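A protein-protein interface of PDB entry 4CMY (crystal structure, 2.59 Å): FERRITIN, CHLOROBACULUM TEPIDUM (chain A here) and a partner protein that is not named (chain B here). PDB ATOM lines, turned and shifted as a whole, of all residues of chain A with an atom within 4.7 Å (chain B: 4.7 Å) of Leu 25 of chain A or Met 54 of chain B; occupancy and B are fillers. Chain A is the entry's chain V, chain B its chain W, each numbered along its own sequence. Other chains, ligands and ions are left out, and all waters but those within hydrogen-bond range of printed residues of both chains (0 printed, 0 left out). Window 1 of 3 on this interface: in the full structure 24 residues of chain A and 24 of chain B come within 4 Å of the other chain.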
ATOM      1  N   ALA A  21      22.825 -24.064 -10.946  1.00  0.00           N
ATOM      2  CA  ALA A  21      23.179 -22.796 -11.514  1.00  0.00           C
ATOM      3  C   ALA A  21      23.220 -21.727 -10.457  1.00  0.00           C
ATOM      4  O   ALA A  21      24.173 -20.954 -10.368  1.00  0.00           O
ATOM      5  CB  ALA A  21      22.200 -22.407 -12.592  1.00  0.00           C
ATOM      6  N   HIS A  22      22.191 -21.702  -9.620  1.00  0.00           N
ATOM      7  CA  HIS A  22      22.087 -20.686  -8.550  1.00  0.00           C
ATOM      8  C   HIS A  22      23.178 -20.888  -7.513  1.00  0.00           C
ATOM      9  O   HIS A  22      23.752 -19.942  -7.050  1.00  0.00           O
ATOM     10  CB  HIS A  22      20.707 -20.752  -7.903  1.00  0.00           C
ATOM     11  CG  HIS A  22      19.653 -20.109  -8.730  1.00  0.00           C
ATOM     12  ND1 HIS A  22      18.427 -19.725  -8.249  1.00  0.00           N
ATOM     13  CD2 HIS A  22      19.666 -19.762 -10.034  1.00  0.00           C
ATOM     14  CE1 HIS A  22      17.714 -19.196  -9.230  1.00  0.00           C
ATOM     15  NE2 HIS A  22      18.440 -19.223 -10.328  1.00  0.00           N
ATOM     16  N   LEU A  23      23.471 -22.139  -7.191  1.00  0.00           N
ATOM     17  CA  LEU A  23      24.542 -22.455  -6.265  1.00  0.00           C
ATOM     18  C   LEU A  23      25.861 -21.901  -6.773  1.00  0.00           C
ATOM     19  O   LEU A  23      26.600 -21.282  -6.042  1.00  0.00           O
ATOM     20  CB  LEU A  23      24.631 -23.964  -6.029  1.00  0.00           C
ATOM     21  CG  LEU A  23      25.727 -24.427  -5.059  1.00  0.00           C
ATOM     22  CD1 LEU A  23      25.513 -23.861  -3.671  1.00  0.00           C
ATOM     23  CD2 LEU A  23      25.787 -25.952  -4.967  1.00  0.00           C
ATOM     24  N   TYR A  24      26.156 -22.123  -8.043  1.00  0.00           N
ATOM     25  CA  TYR A  24      27.450 -21.720  -8.578  1.00  0.00           C
ATOM     26  C   TYR A  24      27.538 -20.219  -8.749  1.00  0.00           C
ATOM     27  O   TYR A  24      28.588 -19.639  -8.571  1.00  0.00           O
ATOM     28  CB  TYR A  24      27.748 -22.470  -9.886  1.00  0.00           C
ATOM     29  CG  TYR A  24      27.950 -23.994  -9.731  1.00  0.00           C
ATOM     30  CD1 TYR A  24      28.371 -24.551  -8.543  1.00  0.00           C
ATOM     31  CD2 TYR A  24      27.734 -24.856 -10.804  1.00  0.00           C
ATOM     32  CE1 TYR A  24      28.537 -25.910  -8.416  1.00  0.00           C
ATOM     33  CE2 TYR A  24      27.905 -26.202 -10.682  1.00  0.00           C
ATOM     34  CZ  TYR A  24      28.294 -26.728  -9.480  1.00  0.00           C
ATOM     35  OH  TYR A  24      28.447 -28.092  -9.319  1.00  0.00           O
ATOM     36  N   LEU A  25      26.424 -19.575  -9.061  1.00  0.00           N
ATOM     37  CA  LEU A  25      26.375 -18.126  -9.011  1.00  0.00           C
ATOM     38  C   LEU A  25      26.718 -17.627  -7.599  1.00  0.00           C
ATOM     39  O   LEU A  25      27.544 -16.717  -7.450  1.00  0.00           O
ATOM     40  CB  LEU A  25      25.012 -17.621  -9.403  1.00  0.00           C
ATOM     41  CG  LEU A  25      24.800 -16.947 -10.755  1.00  0.00           C
ATOM     42  CD1 LEU A  25      25.892 -17.166 -11.771  1.00  0.00           C
ATOM     43  CD2 LEU A  25      23.465 -17.352 -11.320  1.00  0.00           C
ATOM     44  N   GLN A  26      26.106 -18.231  -6.578  1.00  0.00           N
ATOM     45  CA  GLN A  26      26.326 -17.779  -5.230  1.00  0.00           C
ATOM     46  C   GLN A  26      27.772 -18.002  -4.804  1.00  0.00           C
ATOM     47  O   GLN A  26      28.366 -17.170  -4.122  1.00  0.00           O
ATOM     48  CB  GLN A  26      25.367 -18.480  -4.284  1.00  0.00           C
ATOM     49  CG  GLN A  26      25.315 -17.916  -2.886  1.00  0.00           C
ATOM     50  CD  GLN A  26      24.870 -16.465  -2.870  1.00  0.00           C
ATOM     51  OE1 GLN A  26      23.679 -16.176  -2.810  1.00  0.00           O
ATOM     52  NE2 GLN A  26      25.829 -15.553  -2.900  1.00  0.00           N
ATOM     53  N   MET A  27      28.354 -19.124  -5.230  1.00  0.00           N
ATOM     54  CA  MET A  27      29.755 -19.417  -4.942  1.00  0.00           C
ATOM     55  C   MET A  27      30.636 -18.372  -5.616  1.00  0.00           C
ATOM     56  O   MET A  27      31.585 -17.880  -5.016  1.00  0.00           O
ATOM     57  CB  MET A  27      30.144 -20.811  -5.434  1.00  0.00           C
ATOM     58  CG  MET A  27      29.616 -21.948  -4.593  1.00  0.00           C
ATOM     59  SD  MET A  27      30.052 -23.570  -5.267  1.00  0.00           S
ATOM     60  CE  MET A  27      29.505 -24.646  -3.950  1.00  0.00           C
ATOM     61  N   SER A  28      30.303 -18.021  -6.840  1.00  0.00           N
ATOM     62  CA  SER A  28      31.050 -17.008  -7.547  1.00  0.00           C
ATOM     63  C   SER A  28      31.093 -15.711  -6.757  1.00  0.00           C
ATOM     64  O   SER A  28      32.139 -15.066  -6.656  1.00  0.00           O
ATOM     65  CB  SER A  28      30.406 -16.726  -8.928  1.00  0.00           C
ATOM     66  OG  SER A  28      31.199 -15.819  -9.669  1.00  0.00           O
ATOM     67  N   ALA A  29      29.932 -15.303  -6.239  1.00  0.00           N
ATOM     68  CA  ALA A  29      29.829 -14.041  -5.502  1.00  0.00           C
ATOM     69  C   ALA A  29      30.701 -14.081  -4.244  1.00  0.00           C
ATOM     70  O   ALA A  29      31.393 -13.101  -3.950  1.00  0.00           O
ATOM     71  CB  ALA A  29      28.409 -13.765  -5.124  1.00  0.00           C
ATOM     72  N   PHE A  43      33.233 -20.228 -11.777  1.00  0.00           N
ATOM     73  CA  PHE A  43      31.916 -20.607 -11.264  1.00  0.00           C
ATOM     74  C   PHE A  43      30.798 -19.851 -11.936  1.00  0.00           C
ATOM     75  O   PHE A  43      29.747 -20.412 -12.204  1.00  0.00           O
ATOM     76  CB  PHE A  43      31.834 -20.498  -9.766  1.00  0.00           C
ATOM     77  CG  PHE A  43      32.396 -21.689  -9.076  1.00  0.00           C
ATOM     78  CD1 PHE A  43      31.604 -22.793  -8.829  1.00  0.00           C
ATOM     79  CD2 PHE A  43      33.712 -21.725  -8.698  1.00  0.00           C
ATOM     80  CE1 PHE A  43      32.111 -23.890  -8.171  1.00  0.00           C
ATOM     81  CE2 PHE A  43      34.231 -22.827  -8.062  1.00  0.00           C
ATOM     82  CZ  PHE A  43      33.427 -23.916  -7.812  1.00  0.00           C
ATOM     83  N   ARG A  44      31.052 -18.612 -12.298  1.00  0.00           N
ATOM     84  CA  ARG A  44      30.072 -17.863 -13.070  1.00  0.00           C
ATOM     85  C   ARG A  44      29.795 -18.500 -14.430  1.00  0.00           C
ATOM     86  O   ARG A  44      28.657 -18.667 -14.824  1.00  0.00           O
ATOM     87  CB  ARG A  44      30.549 -16.435 -13.308  1.00  0.00           C
ATOM     88  CG  ARG A  44      29.484 -15.603 -13.999  1.00  0.00           C
ATOM     89  CD  ARG A  44      30.093 -14.369 -14.603  1.00  0.00           C
ATOM     90  NE  ARG A  44      29.166 -13.396 -15.119  1.00  0.00           N
ATOM     91  CZ  ARG A  44      28.607 -12.379 -14.501  1.00  0.00           C
ATOM     92  NH1 ARG A  44      28.830 -12.159 -13.221  1.00  0.00           N
ATOM     93  NH2 ARG A  44      27.789 -11.578 -15.189  1.00  0.00           N
ATOM     94  N   ALA A  47      27.842 -21.737 -14.040  1.00  0.00           N
ATOM     95  CA  ALA A  47      26.430 -21.567 -13.782  1.00  0.00           C
ATOM     96  C   ALA A  47      25.689 -21.566 -15.127  1.00  0.00           C
ATOM     97  O   ALA A  47      24.585 -22.054 -15.217  1.00  0.00           O
ATOM     98  CB  ALA A  47      26.170 -20.302 -13.034  1.00  0.00           C
ATOM     99  N   VAL B  14      17.632  -8.650  -7.434  1.00  0.00           N
ATOM    100  CA  VAL B  14      18.302  -9.782  -8.037  1.00  0.00           C
ATOM    101  C   VAL B  14      17.356 -10.971  -8.019  1.00  0.00           C
ATOM    102  O   VAL B  14      17.149 -11.648  -9.005  1.00  0.00           O
ATOM    103  CB  VAL B  14      19.584 -10.160  -7.291  1.00  0.00           C
ATOM    104  CG1 VAL B  14      20.051 -11.519  -7.720  1.00  0.00           C
ATOM    105  CG2 VAL B  14      20.676  -9.148  -7.544  1.00  0.00           C
ATOM    106  N   GLU B  17      14.296 -10.584 -10.412  1.00  0.00           N
ATOM    107  CA  GLU B  17      14.617 -10.838 -11.816  1.00  0.00           C
ATOM    108  C   GLU B  17      14.772 -12.356 -12.030  1.00  0.00           C
ATOM    109  O   GLU B  17      14.301 -12.908 -13.028  1.00  0.00           O
ATOM    110  CB  GLU B  17      15.870 -10.079 -12.262  1.00  0.00           C
ATOM    111  CG  GLU B  17      15.761  -8.585 -12.115  1.00  0.00           C
ATOM    112  CD  GLU B  17      14.802  -7.883 -13.101  1.00  0.00           C
ATOM    113  OE1 GLU B  17      14.474  -8.428 -14.197  1.00  0.00           O
ATOM    114  OE2 GLU B  17      14.419  -6.707 -12.805  1.00  0.00           O
ATOM    115  N   ALA B  18      15.407 -13.041 -11.087  1.00  0.00           N
ATOM    116  CA  ALA B  18      15.533 -14.505 -11.169  1.00  0.00           C
ATOM    117  C   ALA B  18      14.173 -15.182 -11.203  1.00  0.00           C
ATOM    118  O   ALA B  18      13.963 -16.085 -12.006  1.00  0.00           O
ATOM    119  CB  ALA B  18      16.336 -15.036 -10.003  1.00  0.00           C
ATOM    120  N   GLU B  50      15.546 -11.783 -18.827  1.00  0.00           N
ATOM    121  CA  GLU B  50      15.410 -11.553 -17.385  1.00  0.00           C
ATOM    122  C   GLU B  50      16.651 -12.048 -16.657  1.00  0.00           C
ATOM    123  O   GLU B  50      17.084 -11.437 -15.701  1.00  0.00           O
ATOM    124  CB  GLU B  50      14.141 -12.176 -16.832  1.00  0.00           C
ATOM    125  CG  GLU B  50      12.850 -11.596 -17.406  1.00  0.00           C
ATOM    126  CD  GLU B  50      12.594 -10.106 -17.104  1.00  0.00           C
ATOM    127  OE1 GLU B  50      13.298  -9.546 -16.216  1.00  0.00           O
ATOM    128  OE2 GLU B  50      11.626  -9.528 -17.751  1.00  0.00           O
ATOM    129  N   LYS B  51      17.271 -13.097 -17.161  1.00  0.00           N
ATOM    130  CA  LYS B  51      18.524 -13.554 -16.626  1.00  0.00           C
ATOM    131  C   LYS B  51      19.591 -12.483 -16.779  1.00  0.00           C
ATOM    132  O   LYS B  51      20.399 -12.326 -15.899  1.00  0.00           O
ATOM    133  CB  LYS B  51      18.985 -14.836 -17.341  1.00  0.00           C
ATOM    134  CG  LYS B  51      19.398 -15.997 -16.470  1.00  0.00           C
ATOM    135  CD  LYS B  51      18.188 -16.956 -16.398  1.00  0.00           C
ATOM    136  CE  LYS B  51      18.173 -17.980 -15.253  1.00  0.00           C
ATOM    137  NZ  LYS B  51      16.852 -18.507 -14.821  1.00  0.00           N
ATOM    138  N   ALA B  52      19.631 -11.812 -17.912  1.00  0.00           N
ATOM    139  CA  ALA B  52      20.616 -10.772 -18.116  1.00  0.00           C
ATOM    140  C   ALA B  52      20.364  -9.611 -17.155  1.00  0.00           C
ATOM    141  O   ALA B  52      21.325  -9.032 -16.653  1.00  0.00           O
ATOM    142  CB  ALA B  52      20.618 -10.274 -19.563  1.00  0.00           C
ATOM    143  N   HIS B  53      19.090  -9.267 -16.923  1.00  0.00           N
ATOM    144  CA  HIS B  53      18.795  -8.236 -15.951  1.00  0.00           C
ATOM    145  C   HIS B  53      19.346  -8.632 -14.578  1.00  0.00           C
ATOM    146  O   HIS B  53      19.868  -7.812 -13.864  1.00  0.00           O
ATOM    147  CB  HIS B  53      17.286  -7.986 -15.808  1.00  0.00           C
ATOM    148  CG  HIS B  53      16.624  -7.498 -17.051  1.00  0.00           C
ATOM    149  ND1 HIS B  53      15.256  -7.412 -17.173  1.00  0.00           N
ATOM    150  CD2 HIS B  53      17.137  -7.135 -18.247  1.00  0.00           C
ATOM    151  CE1 HIS B  53      14.951  -7.015 -18.394  1.00  0.00           C
ATOM    152  NE2 HIS B  53      16.076  -6.823 -19.060  1.00  0.00           N
ATOM    153  N   MET B  54      19.149  -9.883 -14.209  1.00  0.00           N
ATOM    154  CA  MET B  54      19.613 -10.387 -12.953  1.00  0.00           C
ATOM    155  C   MET B  54      21.112 -10.249 -12.843  1.00  0.00           C
ATOM    156  O   MET B  54      21.610  -9.773 -11.831  1.00  0.00           O
ATOM    157  CB  MET B  54      19.212 -11.857 -12.778  1.00  0.00           C
ATOM    158  CG  MET B  54      19.729 -12.496 -11.499  1.00  0.00           C
ATOM    159  SD  MET B  54      19.475 -14.277 -11.459  1.00  0.00           S
ATOM    160  CE  MET B  54      20.831 -14.745 -12.491  1.00  0.00           C
ATOM    161  N   MET B  55      21.837 -10.672 -13.879  1.00  0.00           N
ATOM    162  CA  MET B  55      23.311 -10.749 -13.809  1.00  0.00           C
ATOM    163  C   MET B  55      23.926  -9.397 -13.732  1.00  0.00           C
ATOM    164  O   MET B  55      24.961  -9.198 -13.117  1.00  0.00           O
ATOM    165  CB  MET B  55      23.864 -11.493 -15.009  1.00  0.00           C
ATOM    166  CG  MET B  55      23.512 -12.989 -15.032  1.00  0.00           C
ATOM    167  SD  MET B  55      23.927 -13.794 -13.488  1.00  0.00           S
ATOM    168  CE  MET B  55      25.723 -13.697 -13.627  1.00  0.00           C
ATOM    169  N   LYS B  56      23.276  -8.429 -14.332  1.00  0.00           N
ATOM    170  CA  LYS B  56      23.813  -7.095 -14.350  1.00  0.00           C
ATOM    171  C   LYS B  56      23.737  -6.471 -12.939  1.00  0.00           C
ATOM    172  O   LYS B  56      24.666  -5.774 -12.519  1.00  0.00           O
ATOM    173  CB  LYS B  56      23.086  -6.307 -15.426  1.00  0.00           C
ATOM    174  CG  LYS B  56      23.292  -4.820 -15.403  1.00  0.00           C
ATOM    175  CD  LYS B  56      22.791  -4.194 -16.703  1.00  0.00           C
ATOM    176  CE  LYS B  56      22.828  -2.681 -16.607  1.00  0.00           C
ATOM    177  NZ  LYS B  56      23.888  -2.093 -17.483  1.00  0.00           N
ATOM    178  N   LEU B  57      22.628  -6.707 -12.230  1.00  0.00           N
ATOM    179  CA  LEU B  57      22.479  -6.308 -10.844  1.00  0.00           C
ATOM    180  C   LEU B  57      23.512  -7.035  -9.994  1.00  0.00           C
ATOM    181  O   LEU B  57      24.165  -6.452  -9.124  1.00  0.00           O
ATOM    182  CB  LEU B  57      21.098  -6.701 -10.303  1.00  0.00           C
ATOM    183  CG  LEU B  57      19.899  -5.820 -10.074  1.00  0.00           C
ATOM    184  CD1 LEU B  57      20.215  -4.353 -10.021  1.00  0.00           C
ATOM    185  CD2 LEU B  57      18.770  -6.045 -11.021  1.00  0.00           C
ATOM    186  N   PHE B  58      23.551  -8.341 -10.162  1.00  0.00           N
ATOM    187  CA  PHE B  58      24.454  -9.207  -9.439  1.00  0.00           C
ATOM    188  C   PHE B  58      25.867  -8.655  -9.555  1.00  0.00           C
ATOM    189  O   PHE B  58      26.584  -8.569  -8.566  1.00  0.00           O
ATOM    190  CB  PHE B  58      24.292 -10.608 -10.047  1.00  0.00           C
ATOM    191  CG  PHE B  58      25.204 -11.670  -9.512  1.00  0.00           C
ATOM    192  CD1 PHE B  58      26.431 -11.939 -10.135  1.00  0.00           C
ATOM    193  CD2 PHE B  58      24.793 -12.503  -8.470  1.00  0.00           C
ATOM    194  CE1 PHE B  58      27.237 -12.975  -9.689  1.00  0.00           C
ATOM    195  CE2 PHE B  58      25.607 -13.544  -8.022  1.00  0.00           C
ATOM    196  CZ  PHE B  58      26.818 -13.784  -8.639  1.00  0.00           C
ATOM    197  N   ILE B  70      21.277 -14.611  -4.128  1.00  0.00           N
ATOM    198  CA  ILE B  70      20.248 -15.076  -5.035  1.00  0.00           C
ATOM    199  C   ILE B  70      18.915 -15.332  -4.304  1.00  0.00           C
ATOM    200  O   ILE B  70      17.847 -14.937  -4.795  1.00  0.00           O
ATOM    201  CB  ILE B  70      20.628 -16.396  -5.716  1.00  0.00           C
ATOM    202  CG1 ILE B  70      22.017 -16.328  -6.318  1.00  0.00           C
ATOM    203  CG2 ILE B  70      19.596 -16.714  -6.811  1.00  0.00           C
ATOM    204  CD1 ILE B  70      22.137 -15.409  -7.509  1.00  0.00           C
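The side-chain amide oxygen of Gln 26 of chain A is in hydrogen-bond range of the backbone NH of Ile 70 of chain B.
Among the printed residues, pairs that only touch across the chains: Leu 25 of chain A with Phe 58 of chain B, Arg 44 of chain A with Met 55 of chain B, His 22 of chain A with Ile 70 of chain B, Ala 29 of chain A with Phe 58 of chain B, Leu 25 of chain A with Met 54 of chain B, Arg 44 of chain A with Phe 58 of chain B and Leu 25 of chain A with Met 55 of chain B.
Met 54 of chain B touches just one residue of chain A: Leu 25 (3.9 Å). Printed residues of chain B within 4 Å of Gln 26 of chain A: Ile 70 (3.2 Å). Of the printed residues of chain B, Arg 44 of chain A touches Met 55 (3.3 Å) and Phe 58 (3.9 Å). Printed residues of chain A within 4 Å of Ile 70 of chain B: His 22 (3.5 Å) and Gln 26 (3.2 Å). Of the printed residues of chain A, Met 55 of chain B touches Leu 25 and Arg 44. Of the printed residues of chain B, Ala 29 of chain A touches Phe 58 (3.9 Å). The nearest printed residue of chain B that does not touch Gln 26 of chain A is Phe 58 of chain B (4.9 Å).
Printed residues of chain A that touch a printed residue of chain B: His 22, Leu 25, Gln 26, Ala 29 and Arg 44. Of the 13 printed residues of chain B, 4 touch a printed residue of chain A. Printed residues of chain B that touch a printed residue of chain A: Met 54, Met 55, Phe 58 and Ile 70. Hydrophobic or aromatic side chains of chain B within 4 Å of the printed part of chain A: Met 54, Met 55, Phe 58 and Ile 70. Among the printed residues, no Asp or Glu carboxylate lies within 4 Å of a Lys or Arg side-chain nitrogen of the other chain.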
